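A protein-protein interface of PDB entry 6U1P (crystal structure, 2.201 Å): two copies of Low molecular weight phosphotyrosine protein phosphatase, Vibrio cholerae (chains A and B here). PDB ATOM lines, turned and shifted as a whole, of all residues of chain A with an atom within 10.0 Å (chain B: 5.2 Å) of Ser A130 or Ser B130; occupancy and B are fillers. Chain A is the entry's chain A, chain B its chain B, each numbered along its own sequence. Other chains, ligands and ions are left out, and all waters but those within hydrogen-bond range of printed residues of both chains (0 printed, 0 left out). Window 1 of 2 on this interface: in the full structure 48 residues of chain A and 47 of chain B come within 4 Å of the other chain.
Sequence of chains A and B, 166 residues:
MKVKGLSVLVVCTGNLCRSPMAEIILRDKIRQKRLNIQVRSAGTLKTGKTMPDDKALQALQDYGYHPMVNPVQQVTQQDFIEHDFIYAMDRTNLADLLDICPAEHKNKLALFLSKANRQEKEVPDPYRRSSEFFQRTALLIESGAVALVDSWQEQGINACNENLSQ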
ATOM      1  N   CYS A  17      17.885  23.078  11.689  1.00  0.00           N
ATOM      2  CA  CYS A  17      17.443  22.097  10.703  1.00  0.00           C
ATOM      3  C   CYS A  17      17.016  22.749   9.401  1.00  0.00           C
ATOM      4  O   CYS A  17      17.787  22.786   8.433  1.00  0.00           O
ATOM      5  CB  CYS A  17      16.272  21.278  11.255  1.00  0.00           C
ATOM      6  SG  CYS A  17      16.692  20.288  12.681  1.00  0.00           S
ATOM      7  N   MET A  21      19.580  23.832   6.240  1.00  0.00           N
ATOM      8  CA  MET A  21      19.382  23.033   5.039  1.00  0.00           C
ATOM      9  C   MET A  21      19.122  23.929   3.844  1.00  0.00           C
ATOM     10  O   MET A  21      19.719  23.755   2.774  1.00  0.00           O
ATOM     11  CB  MET A  21      18.228  22.057   5.224  1.00  0.00           C
ATOM     12  CG  MET A  21      18.607  20.875   6.112  1.00  0.00           C
ATOM     13  SD  MET A  21      17.158  19.840   6.467  1.00  0.00           S
ATOM     14  CE  MET A  21      17.275  18.653   5.157  1.00  0.00           C
ATOM     15  N   ASP A  53      22.070  20.398  13.352  1.00  0.00           N
ATOM     16  CA  ASP A  53      21.772  19.000  13.670  1.00  0.00           C
ATOM     17  C   ASP A  53      22.426  18.013  12.702  1.00  0.00           C
ATOM     18  O   ASP A  53      22.323  18.143  11.474  1.00  0.00           O
ATOM     19  CB  ASP A  53      20.249  18.803  13.654  1.00  0.00           C
ATOM     20  CG  ASP A  53      19.806  17.421  14.156  1.00  0.00           C
ATOM     21  OD1 ASP A  53      20.409  16.391  13.775  1.00  0.00           O
ATOM     22  OD2 ASP A  53      18.822  17.368  14.920  1.00  0.00           O
ATOM     23  N   ASP A  54      23.011  16.959  13.276  1.00  0.00           N
ATOM     24  CA  ASP A  54      23.656  15.911  12.489  1.00  0.00           C
ATOM     25  C   ASP A  54      22.721  15.318  11.440  1.00  0.00           C
ATOM     26  O   ASP A  54      23.152  15.012  10.322  1.00  0.00           O
ATOM     27  CB  ASP A  54      24.139  14.789  13.413  1.00  0.00           C
ATOM     28  CG  ASP A  54      25.544  15.012  13.927  1.00  0.00           C
ATOM     29  OD1 ASP A  54      26.183  16.009  13.525  1.00  0.00           O
ATOM     30  OD2 ASP A  54      26.008  14.182  14.742  1.00  0.00           O
ATOM     31  N   LYS A  55      21.449  15.104  11.784  1.00  0.00           N
ATOM     32  CA  LYS A  55      20.577  14.466  10.809  1.00  0.00           C
ATOM     33  C   LYS A  55      20.080  15.444   9.756  1.00  0.00           C
ATOM     34  O   LYS A  55      19.699  15.009   8.668  1.00  0.00           O
ATOM     35  CB  LYS A  55      19.428  13.723  11.488  1.00  0.00           C
ATOM     36  CG  LYS A  55      18.376  14.560  12.152  1.00  0.00           C
ATOM     37  CD  LYS A  55      17.598  13.723  13.185  1.00  0.00           C
ATOM     38  CE  LYS A  55      18.502  12.773  13.930  1.00  0.00           C
ATOM     39  NZ  LYS A  55      17.697  11.780  14.721  1.00  0.00           N
ATOM     40  N   ALA A  56      20.083  16.751  10.022  1.00  0.00           N
ATOM     41  CA  ALA A  56      19.904  17.686   8.910  1.00  0.00           C
ATOM     42  C   ALA A  56      21.025  17.513   7.892  1.00  0.00           C
ATOM     43  O   ALA A  56      20.783  17.438   6.681  1.00  0.00           O
ATOM     44  CB  ALA A  56      19.873  19.133   9.419  1.00  0.00           C
ATOM     45  N   GLN A  58      23.125  14.950   7.387  1.00  0.00           N
ATOM     46  CA  GLN A  58      23.167  13.650   6.735  1.00  0.00           C
ATOM     47  C   GLN A  58      22.073  13.549   5.699  1.00  0.00           C
ATOM     48  O   GLN A  58      22.280  12.978   4.623  1.00  0.00           O
ATOM     49  CB  GLN A  58      23.025  12.531   7.768  1.00  0.00           C
ATOM     50  CG  GLN A  58      24.279  12.319   8.579  1.00  0.00           C
ATOM     51  CD  GLN A  58      24.019  11.735   9.959  1.00  0.00           C
ATOM     52  OE1 GLN A  58      22.919  11.834  10.508  1.00  0.00           O
ATOM     53  NE2 GLN A  58      25.044  11.126  10.527  1.00  0.00           N
ATOM     54  N   ALA A  59      20.905  14.118   5.999  1.00  0.00           N
ATOM     55  CA  ALA A  59      19.845  14.143   5.005  1.00  0.00           C
ATOM     56  C   ALA A  59      20.276  14.927   3.765  1.00  0.00           C
ATOM     57  O   ALA A  59      19.866  14.598   2.646  1.00  0.00           O
ATOM     58  CB  ALA A  59      18.577  14.724   5.621  1.00  0.00           C
ATOM     59  N   ASP A  62      22.507  12.575   1.882  1.00  0.00           N
ATOM     60  CA  ASP A  62      21.736  11.517   1.231  1.00  0.00           C
ATOM     61  C   ASP A  62      21.262  11.941  -0.154  1.00  0.00           C
ATOM     62  O   ASP A  62      21.030  11.090  -1.016  1.00  0.00           O
ATOM     63  CB  ASP A  62      20.537  11.097   2.093  1.00  0.00           C
ATOM     64  CG  ASP A  62      20.944  10.407   3.406  1.00  0.00           C
ATOM     65  OD1 ASP A  62      22.118   9.976   3.562  1.00  0.00           O
ATOM     66  OD2 ASP A  62      20.060  10.309   4.289  1.00  0.00           O
ATOM     67  N   PRO A 124       7.220  22.008   7.291  1.00  0.00           N
ATOM     68  CA  PRO A 124       6.948  21.552   8.674  1.00  0.00           C
ATOM     69  C   PRO A 124       8.245  21.244   9.400  1.00  0.00           C
ATOM     70  O   PRO A 124       9.252  20.889   8.788  1.00  0.00           O
ATOM     71  CB  PRO A 124       6.114  20.266   8.499  1.00  0.00           C
ATOM     72  CG  PRO A 124       5.607  20.310   7.077  1.00  0.00           C
ATOM     73  CD  PRO A 124       6.615  21.125   6.274  1.00  0.00           C
ATOM     74  N   ASP A 125       8.230  21.461  10.704  1.00  0.00           N
ATOM     75  CA  ASP A 125       9.407  21.301  11.551  1.00  0.00           C
ATOM     76  C   ASP A 125       9.721  19.823  11.792  1.00  0.00           C
ATOM     77  O   ASP A 125       8.975  19.157  12.529  1.00  0.00           O
ATOM     78  CB  ASP A 125       9.147  22.027  12.874  1.00  0.00           C
ATOM     79  CG  ASP A 125      10.310  21.945  13.857  1.00  0.00           C
ATOM     80  OD1 ASP A 125      11.345  21.296  13.560  1.00  0.00           O
ATOM     81  OD2 ASP A 125      10.181  22.579  14.937  1.00  0.00           O
ATOM     82  N   PRO A 126      10.846  19.305  11.303  1.00  0.00           N
ATOM     83  CA  PRO A 126      11.150  17.885  11.536  1.00  0.00           C
ATOM     84  C   PRO A 126      11.324  17.561  13.002  1.00  0.00           C
ATOM     85  O   PRO A 126      11.013  16.440  13.418  1.00  0.00           O
ATOM     86  CB  PRO A 126      12.455  17.660  10.748  1.00  0.00           C
ATOM     87  CG  PRO A 126      12.715  18.924  10.000  1.00  0.00           C
ATOM     88  CD  PRO A 126      11.955  20.018  10.655  1.00  0.00           C
ATOM     89  N   TYR A 127      11.784  18.527  13.800  1.00  0.00           N
ATOM     90  CA  TYR A 127      11.998  18.302  15.228  1.00  0.00           C
ATOM     91  C   TYR A 127      10.691  18.055  15.953  1.00  0.00           C
ATOM     92  O   TYR A 127      10.620  17.195  16.836  1.00  0.00           O
ATOM     93  CB  TYR A 127      12.700  19.506  15.863  1.00  0.00           C
ATOM     94  CG  TYR A 127      14.184  19.344  16.039  1.00  0.00           C
ATOM     95  CD1 TYR A 127      14.711  18.237  16.680  1.00  0.00           C
ATOM     96  CD2 TYR A 127      15.057  20.325  15.600  1.00  0.00           C
ATOM     97  CE1 TYR A 127      16.070  18.089  16.852  1.00  0.00           C
ATOM     98  CE2 TYR A 127      16.416  20.197  15.782  1.00  0.00           C
ATOM     99  CZ  TYR A 127      16.919  19.074  16.396  1.00  0.00           C
ATOM    100  OH  TYR A 127      18.282  18.954  16.559  1.00  0.00           O
ATOM    101  N   ARG A 128       9.646  18.813  15.619  1.00  0.00           N
ATOM    102  CA  ARG A 128       8.380  18.593  16.303  1.00  0.00           C
ATOM    103  C   ARG A 128       7.769  17.249  15.924  1.00  0.00           C
ATOM    104  O   ARG A 128       7.270  16.528  16.793  1.00  0.00           O
ATOM    105  CB  ARG A 128       7.397  19.724  15.991  1.00  0.00           C
ATOM    106  CG  ARG A 128       6.050  19.555  16.707  1.00  0.00           C
ATOM    107  CD  ARG A 128       4.867  20.165  15.960  1.00  0.00           C
ATOM    108  NE  ARG A 128       4.891  19.907  14.522  1.00  0.00           N
ATOM    109  CZ  ARG A 128       4.792  18.708  13.956  1.00  0.00           C
ATOM    110  NH1 ARG A 128       4.650  17.613  14.696  1.00  0.00           N
ATOM    111  NH2 ARG A 128       4.830  18.615  12.637  1.00  0.00           N
ATOM    112  N   ARG A 129       7.807  16.890  14.640  1.00  0.00           N
ATOM    113  CA  ARG A 129       7.356  15.563  14.235  1.00  0.00           C
ATOM    114  C   ARG A 129       8.147  14.480  14.953  1.00  0.00           C
ATOM    115  O   ARG A 129       7.576  13.543  15.521  1.00  0.00           O
ATOM    116  CB  ARG A 129       7.479  15.405  12.711  1.00  0.00           C
ATOM    117  CG  ARG A 129       6.424  14.504  12.054  1.00  0.00           C
ATOM    118  CD  ARG A 129       5.954  15.033  10.662  1.00  0.00           C
ATOM    119  NE  ARG A 129       5.318  16.356  10.715  1.00  0.00           N
ATOM    120  CZ  ARG A 129       4.658  16.942   9.708  1.00  0.00           C
ATOM    121  NH1 ARG A 129       4.532  16.344   8.528  1.00  0.00           N
ATOM    122  NH2 ARG A 129       4.110  18.139   9.882  1.00  0.00           N
ATOM    123  N   SER A 130       9.473  14.609  14.960  1.00  0.00           N
ATOM    124  CA  SER A 130      10.296  13.624  15.646  1.00  0.00           C
ATOM    125  C   SER A 130       9.875  13.477  17.104  1.00  0.00           C
ATOM    126  O   SER A 130       9.715  12.359  17.608  1.00  0.00           O
ATOM    127  CB  SER A 130      11.767  13.991  15.533  1.00  0.00           C
ATOM    128  OG  SER A 130      12.529  12.837  15.843  1.00  0.00           O
ATOM    129  N   SER A 131       9.706  14.603  17.798  1.00  0.00           N
ATOM    130  CA  SER A 131       9.289  14.583  19.198  1.00  0.00           C
ATOM    131  C   SER A 131       7.965  13.849  19.367  1.00  0.00           C
ATOM    132  O   SER A 131       7.787  13.079  20.320  1.00  0.00           O
ATOM    133  CB  SER A 131       9.164  16.015  19.723  1.00  0.00           C
ATOM    134  OG  SER A 131      10.422  16.669  19.697  1.00  0.00           O
ATOM    135  N   GLU A 132       7.015  14.107  18.469  1.00  0.00           N
ATOM    136  CA  GLU A 132       5.747  13.389  18.501  1.00  0.00           C
ATOM    137  C   GLU A 132       5.973  11.891  18.411  1.00  0.00           C
ATOM    138  O   GLU A 132       5.363  11.119  19.156  1.00  0.00           O
ATOM    139  CB  GLU A 132       4.842  13.879  17.366  1.00  0.00           C
ATOM    140  CG  GLU A 132       3.643  13.015  17.023  1.00  0.00           C
ATOM    141  CD  GLU A 132       2.513  13.264  18.019  1.00  0.00           C
ATOM    142  OE1 GLU A 132       1.429  13.709  17.613  1.00  0.00           O
ATOM    143  OE2 GLU A 132       2.683  12.997  19.218  1.00  0.00           O
ATOM    144  N   PHE A 133       6.896  11.462  17.554  1.00  0.00           N
ATOM    145  CA  PHE A 133       7.030  10.029  17.334  1.00  0.00           C
ATOM    146  C   PHE A 133       7.706   9.344  18.521  1.00  0.00           C
ATOM    147  O   PHE A 133       7.314   8.238  18.905  1.00  0.00           O
ATOM    148  CB  PHE A 133       7.787   9.770  16.033  1.00  0.00           C
ATOM    149  CG  PHE A 133       7.675   8.368  15.562  1.00  0.00           C
ATOM    150  CD1 PHE A 133       6.545   7.948  14.859  1.00  0.00           C
ATOM    151  CD2 PHE A 133       8.668   7.442  15.859  1.00  0.00           C
ATOM    152  CE1 PHE A 133       6.414   6.630  14.433  1.00  0.00           C
ATOM    153  CE2 PHE A 133       8.543   6.115  15.442  1.00  0.00           C
ATOM    154  CZ  PHE A 133       7.414   5.713  14.725  1.00  0.00           C
ATOM    155  N   PHE A 134       8.681  10.012  19.152  1.00  0.00           N
ATOM    156  CA  PHE A 134       9.273   9.454  20.362  1.00  0.00           C
ATOM    157  C   PHE A 134       8.236   9.330  21.469  1.00  0.00           C
ATOM    158  O   PHE A 134       8.234   8.345  22.219  1.00  0.00           O
ATOM    159  CB  PHE A 134      10.449  10.300  20.842  1.00  0.00           C
ATOM    160  CG  PHE A 134      11.753   9.978  20.165  1.00  0.00           C
ATOM    161  CD1 PHE A 134      12.113  10.613  18.987  1.00  0.00           C
ATOM    162  CD2 PHE A 134      12.629   9.042  20.707  1.00  0.00           C
ATOM    163  CE1 PHE A 134      13.316  10.326  18.351  1.00  0.00           C
ATOM    164  CE2 PHE A 134      13.845   8.752  20.070  1.00  0.00           C
ATOM    165  CZ  PHE A 134      14.179   9.391  18.894  1.00  0.00           C
ATOM    166  N   GLN A 135       7.330  10.310  21.580  1.00  0.00           N
ATOM    167  CA  GLN A 135       6.252  10.181  22.564  1.00  0.00           C
ATOM    168  C   GLN A 135       5.370   8.975  22.269  1.00  0.00           C
ATOM    169  O   GLN A 135       5.056   8.188  23.176  1.00  0.00           O
ATOM    170  CB  GLN A 135       5.394  11.436  22.606  1.00  0.00           C
ATOM    171  CG  GLN A 135       6.127  12.666  23.090  1.00  0.00           C
ATOM    172  CD  GLN A 135       5.258  13.915  22.992  1.00  0.00           C
ATOM    173  OE1 GLN A 135       4.389  14.015  22.115  1.00  0.00           O
ATOM    174  NE2 GLN A 135       5.489  14.870  23.888  1.00  0.00           N
ATOM    175  N   ARG A 136       4.984   8.785  21.007  1.00  0.00           N
ATOM    176  CA  ARG A 136       4.150   7.624  20.734  1.00  0.00           C
ATOM    177  C   ARG A 136       4.992   6.361  20.866  1.00  0.00           C
ATOM    178  O   ARG A 136       4.469   5.326  21.257  1.00  0.00           O
ATOM    179  CB  ARG A 136       3.454   7.721  19.373  1.00  0.00           C
ATOM    180  CG  ARG A 136       2.851   9.102  19.106  1.00  0.00           C
ATOM    181  CD  ARG A 136       2.278   9.361  17.680  1.00  0.00           C
ATOM    182  NE  ARG A 136       1.067  10.209  17.620  1.00  0.00           N
ATOM    183  CZ  ARG A 136       0.845  11.053  16.608  1.00  0.00           C
ATOM    184  NH1 ARG A 136       1.697  11.072  15.607  1.00  0.00           N
ATOM    185  NH2 ARG A 136      -0.187  11.895  16.597  1.00  0.00           N
ATOM    186  N   THR A 137       6.308   6.431  20.604  1.00  0.00           N
ATOM    187  CA  THR A 137       7.128   5.244  20.837  1.00  0.00           C
ATOM    188  C   THR A 137       7.124   4.874  22.313  1.00  0.00           C
ATOM    189  O   THR A 137       6.945   3.701  22.668  1.00  0.00           O
ATOM    190  CB  THR A 137       8.569   5.445  20.369  1.00  0.00           C
ATOM    191  OG1 THR A 137       8.590   5.778  18.981  1.00  0.00           O
ATOM    192  CG2 THR A 137       9.377   4.165  20.577  1.00  0.00           C
ATOM    193  N   ALA A 138       7.285   5.873  23.185  1.00  0.00           N
ATOM    194  CA  ALA A 138       7.240   5.625  24.621  1.00  0.00           C
ATOM    195  C   ALA A 138       5.916   4.992  25.038  1.00  0.00           C
ATOM    196  O   ALA A 138       5.906   4.051  25.834  1.00  0.00           O
ATOM    197  CB  ALA A 138       7.489   6.917  25.397  1.00  0.00           C
ATOM    198  N   LYS B  55      16.464  12.841  23.060  1.00  0.00           N
ATOM    199  CA  LYS B  55      15.040  12.901  22.754  1.00  0.00           C
ATOM    200  C   LYS B  55      14.291  11.717  23.349  1.00  0.00           C
ATOM    201  O   LYS B  55      13.115  11.844  23.711  1.00  0.00           O
ATOM    202  CB  LYS B  55      14.825  12.927  21.248  1.00  0.00           C
ATOM    203  CG  LYS B  55      15.624  13.960  20.499  1.00  0.00           C
ATOM    204  CD  LYS B  55      15.694  13.543  19.044  1.00  0.00           C
ATOM    205  CE  LYS B  55      14.404  13.908  18.321  1.00  0.00           C
ATOM    206  NZ  LYS B  55      14.449  15.299  17.742  1.00  0.00           N
ATOM    207  N   PRO B 126      12.503   4.828  16.127  1.00  0.00           N
ATOM    208  CA  PRO B 126      12.147   6.223  15.940  1.00  0.00           C
ATOM    209  C   PRO B 126      13.192   6.933  15.087  1.00  0.00           C
ATOM    210  O   PRO B 126      12.866   7.799  14.377  1.00  0.00           O
ATOM    211  CB  PRO B 126      12.201   6.791  17.350  1.00  0.00           C
ATOM    212  CG  PRO B 126      12.184   5.597  18.236  1.00  0.00           C
ATOM    213  CD  PRO B 126      12.914   4.529  17.466  1.00  0.00           C
ATOM    214  N   TYR B 127      14.418   6.464  15.168  1.00  0.00           N
ATOM    215  CA  TYR B 127      15.554   7.044  14.434  1.00  0.00           C
ATOM    216  C   TYR B 127      15.372   6.882  12.923  1.00  0.00           C
ATOM    217  O   TYR B 127      15.705   7.788  12.208  1.00  0.00           O
ATOM    218  CB  TYR B 127      16.822   6.397  14.962  1.00  0.00           C
ATOM    219  CG  TYR B 127      18.027   7.284  15.030  1.00  0.00           C
ATOM    220  CD1 TYR B 127      18.896   7.376  13.958  1.00  0.00           C
ATOM    221  CD2 TYR B 127      18.317   8.003  16.172  1.00  0.00           C
ATOM    222  CE1 TYR B 127      20.023   8.178  14.002  1.00  0.00           C
ATOM    223  CE2 TYR B 127      19.445   8.805  16.239  1.00  0.00           C
ATOM    224  CZ  TYR B 127      20.299   8.892  15.153  1.00  0.00           C
ATOM    225  OH  TYR B 127      21.414   9.676  15.207  1.00  0.00           O
ATOM    226  N   ARG B 128      14.908   5.735  12.448  1.00  0.00           N
ATOM    227  CA  ARG B 128      14.674   5.577  10.996  1.00  0.00           C
ATOM    228  C   ARG B 128      13.513   6.497  10.620  1.00  0.00           C
ATOM    229  O   ARG B 128      13.592   7.141   9.609  1.00  0.00           O
ATOM    230  CB  ARG B 128      14.407   4.110  10.648  1.00  0.00           C
ATOM    231  CG  ARG B 128      13.490   3.886   9.451  1.00  0.00           C
ATOM    232  CD  ARG B 128      13.522   2.506   8.804  1.00  0.00           C
ATOM    233  NE  ARG B 128      12.690   2.318   7.612  1.00  0.00           N
ATOM    234  CZ  ARG B 128      11.356   2.237   7.601  1.00  0.00           C
ATOM    235  NH1 ARG B 128      10.683   2.219   8.736  1.00  0.00           N
ATOM    236  NH2 ARG B 128      10.692   2.167   6.462  1.00  0.00           N
ATOM    237  N   ARG B 129      12.458   6.508  11.416  1.00  0.00           N
ATOM    238  CA  ARG B 129      11.373   7.445  11.127  1.00  0.00           C
ATOM    239  C   ARG B 129      11.903   8.882  11.069  1.00  0.00           C
ATOM    240  O   ARG B 129      11.507   9.684  10.204  1.00  0.00           O
ATOM    241  CB  ARG B 129      10.308   7.308  12.201  1.00  0.00           C
ATOM    242  CG  ARG B 129       8.949   7.867  11.839  1.00  0.00           C
ATOM    243  CD  ARG B 129       8.376   7.176  10.621  1.00  0.00           C
ATOM    244  NE  ARG B 129       7.084   7.729  10.216  1.00  0.00           N
ATOM    245  CZ  ARG B 129       6.924   8.621   9.240  1.00  0.00           C
ATOM    246  NH1 ARG B 129       7.980   9.073   8.573  1.00  0.00           N
ATOM    247  NH2 ARG B 129       5.708   9.065   8.929  1.00  0.00           N
ATOM    248  N   SER B 130      12.759   9.245  12.029  1.00  0.00           N
ATOM    249  CA  SER B 130      13.329  10.584  12.016  1.00  0.00           C
ATOM    250  C   SER B 130      14.006  10.869  10.690  1.00  0.00           C
ATOM    251  O   SER B 130      13.719  11.882  10.045  1.00  0.00           O
ATOM    252  CB  SER B 130      14.301  10.762  13.182  1.00  0.00           C
ATOM    253  OG  SER B 130      14.480  12.155  13.433  1.00  0.00           O
ATOM    254  N   SER B 131      14.890   9.966  10.262  1.00  0.00           N
ATOM    255  CA  SER B 131      15.635  10.168   9.025  1.00  0.00           C
ATOM    256  C   SER B 131      14.712  10.322   7.833  1.00  0.00           C
ATOM    257  O   SER B 131      14.952  11.175   6.968  1.00  0.00           O
ATOM    258  CB  SER B 131      16.602   9.012   8.791  1.00  0.00           C
ATOM    259  OG  SER B 131      17.711   9.117   9.659  1.00  0.00           O
ATOM    260  N   GLU B 132      13.670   9.492   7.749  1.00  0.00           N
ATOM    261  CA  GLU B 132      12.706   9.643   6.663  1.00  0.00           C
ATOM    262  C   GLU B 132      12.139  11.052   6.632  1.00  0.00           C
ATOM    263  O   GLU B 132      12.002  11.653   5.561  1.00  0.00           O
ATOM    264  CB  GLU B 132      11.583   8.621   6.801  1.00  0.00           C
ATOM    265  CG  GLU B 132      12.004   7.186   6.470  1.00  0.00           C
ATOM    266  CD  GLU B 132      10.819   6.248   6.329  1.00  0.00           C
ATOM    267  OE1 GLU B 132      10.744   5.514   5.317  1.00  0.00           O
ATOM    268  OE2 GLU B 132       9.955   6.258   7.231  1.00  0.00           O
ATOM    269  N   PHE B 133      11.836  11.621   7.795  1.00  0.00           N
ATOM    270  CA  PHE B 133      11.189  12.908   7.692  1.00  0.00           C
ATOM    271  C   PHE B 133      12.173  14.015   7.312  1.00  0.00           C
ATOM    272  O   PHE B 133      11.805  14.920   6.548  1.00  0.00           O
ATOM    273  CB  PHE B 133      10.436  13.279   8.958  1.00  0.00           C
ATOM    274  CG  PHE B 133       9.496  14.410   8.723  1.00  0.00           C
ATOM    275  CD1 PHE B 133       8.311  14.192   8.019  1.00  0.00           C
ATOM    276  CD2 PHE B 133       9.840  15.709   9.078  1.00  0.00           C
ATOM    277  CE1 PHE B 133       7.461  15.246   7.726  1.00  0.00           C
ATOM    278  CE2 PHE B 133       8.985  16.767   8.803  1.00  0.00           C
ATOM    279  CZ  PHE B 133       7.800  16.539   8.127  1.00  0.00           C
ATOM    280  N   PHE B 134      13.425  13.931   7.781  1.00  0.00           N
ATOM    281  CA  PHE B 134      14.438  14.914   7.395  1.00  0.00           C
ATOM    282  C   PHE B 134      14.691  14.875   5.891  1.00  0.00           C
ATOM    283  O   PHE B 134      14.888  15.919   5.257  1.00  0.00           O
ATOM    284  CB  PHE B 134      15.738  14.681   8.174  1.00  0.00           C
ATOM    285  CG  PHE B 134      15.746  15.329   9.542  1.00  0.00           C
ATOM    286  CD1 PHE B 134      15.109  14.733  10.622  1.00  0.00           C
ATOM    287  CD2 PHE B 134      16.364  16.541   9.739  1.00  0.00           C
ATOM    288  CE1 PHE B 134      15.089  15.347  11.856  1.00  0.00           C
ATOM    289  CE2 PHE B 134      16.358  17.148  10.977  1.00  0.00           C
ATOM    290  CZ  PHE B 134      15.727  16.555  12.035  1.00  0.00           C
ATOM    291  N   GLN B 135      14.679  13.662   5.330  1.00  0.00           N
ATOM    292  CA  GLN B 135      14.889  13.465   3.871  1.00  0.00           C
ATOM    293  C   GLN B 135      13.708  14.090   3.120  1.00  0.00           C
ATOM    294  O   GLN B 135      13.928  14.646   2.026  1.00  0.00           O
ATOM    295  CB  GLN B 135      15.023  11.976   3.547  1.00  0.00           C
ATOM    296  CG  GLN B 135      16.335  11.365   4.019  1.00  0.00           C
ATOM    297  CD  GLN B 135      16.364   9.867   3.837  1.00  0.00           C
ATOM    298  OE1 GLN B 135      15.350   9.239   3.539  1.00  0.00           O
ATOM    299  NE2 GLN B 135      17.536   9.280   4.017  1.00  0.00           N
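The side-chain amino group (NZ) of Lys A55 is in hydrogen-bond range of the side-chain hydroxyl (OG) of Ser B130 (3.5 Å).
The side-chain amide nitrogen (NE2) of Gln B135 lies within hydrogen-bond range of the side-chain carboxylate (OD2) of Asp A62 (2.7 Å).
OG of Ser B130 sits at hydrogen-bond distance from OG of Ser A130, at 3.2 Å.
OD1 of Asp A53 lies within hydrogen-bond range of N of Lys A55.
N of Tyr A127 lies within hydrogen-bond range of OD1 of Asp A125, 2.8 Å away.
The side-chain hydroxyl (OG) of Ser A131 lies within hydrogen-bond range of the backbone carbonyl oxygen (O) of Tyr A127 (2.9 Å).
The backbone carbonyl oxygen (O) of Phe A133 sits at hydrogen-bond distance from the side-chain hydroxyl (OG1) of Thr A137.
The guanidinium group of Arg B129 lies within salt-bridge range of the side-chain carboxylate of Glu B132, at 3.7 Å.
CE2 of Phe B134 touches SG of Cys A17 (3.6 Å).
Met A21 touches Phe B134.
Lys A55 touches Tyr B127 (NZ to CE2, 3.8 Å).
Ala A56 touches Phe B134 (N to CD2, 3.7 Å).
Ala A59 touches Phe B134 (CB to CB, 3.8 Å).
Phe B133 touches Pro A126.
CE1 of Phe B134 touches CB of Pro A126, at 3.7 Å.
NZ of Lys B55 touches CD1 of Tyr A127 (3.1 Å).
Arg A129 touches Phe B133 (NH1 to CE1, 3.2 Å).
Pro B126 touches Phe A133 (CA to CE2, 3.6 Å).
Asp A53 touches none of the printed residues of chain B.
Of the printed residues of chain B, Tyr A127 touches Lys B55 (3.1 Å).
Ser A130 touches two residues of chain B.
Of the printed residues of chain A, Ser B130 touches Lys A55 and Ser A130.
No residue of chain A comes within 4 Å of Ser B131.
Of the printed residues of chain A, Phe B133 touches Pro A126 (3.5 Å) and Arg A129 (3.2 Å).
The nearest residue of chain B that does not touch Ser A130 is Phe B134 (5.1 Å).
The nearest residue of chain A that does not touch Ser B130 is Phe A134 (5.3 Å).
The nearest printed residue of chain A that does not touch Arg B129 is Arg A129 (6.2 Å).
Printed residues of chain A that touch a printed residue of chain B: Cys A17, Met A21, Lys A55, Ala A56, Ala A59, Asp A62, Pro A126, Tyr A127, Arg A129, Ser A130, Phe A133, Phe A134 and Thr A137.
Hydrophobic or aromatic side chains of chain A that line the printed part of chain B: Met A21, Ala A59, Pro A126, Tyr A127, Phe A133 and Phe A134.
Of the 11 printed residues of chain B, 8 touch a printed residue of chain A.
Printed residues of chain B that touch a printed residue of chain A: Lys B55, Pro B126, Tyr B127, Arg B129, Ser B130, Phe B133, Phe B134 and Gln B135.
Among the printed residues, no Asp or Glu carboxylate lies within 4 Å of a Lys or Arg side-chain nitrogen of the other chain.
Lys A55 touches Phe B134, and with the chains exchanged Phe A134 touches Lys B55.
Pro A126 touches Phe B133, and with the chains exchanged Phe A133 touches Pro B126.
Arg A129 touches Phe B133, and with the chains exchanged Phe A133 touches Arg B129.
Ser A130 touches its own counterpart, Ser B130.
Positions printed for both chains: 55, 126, 127, 128, 129, 130, 131, 132, 133, 134 and 135.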
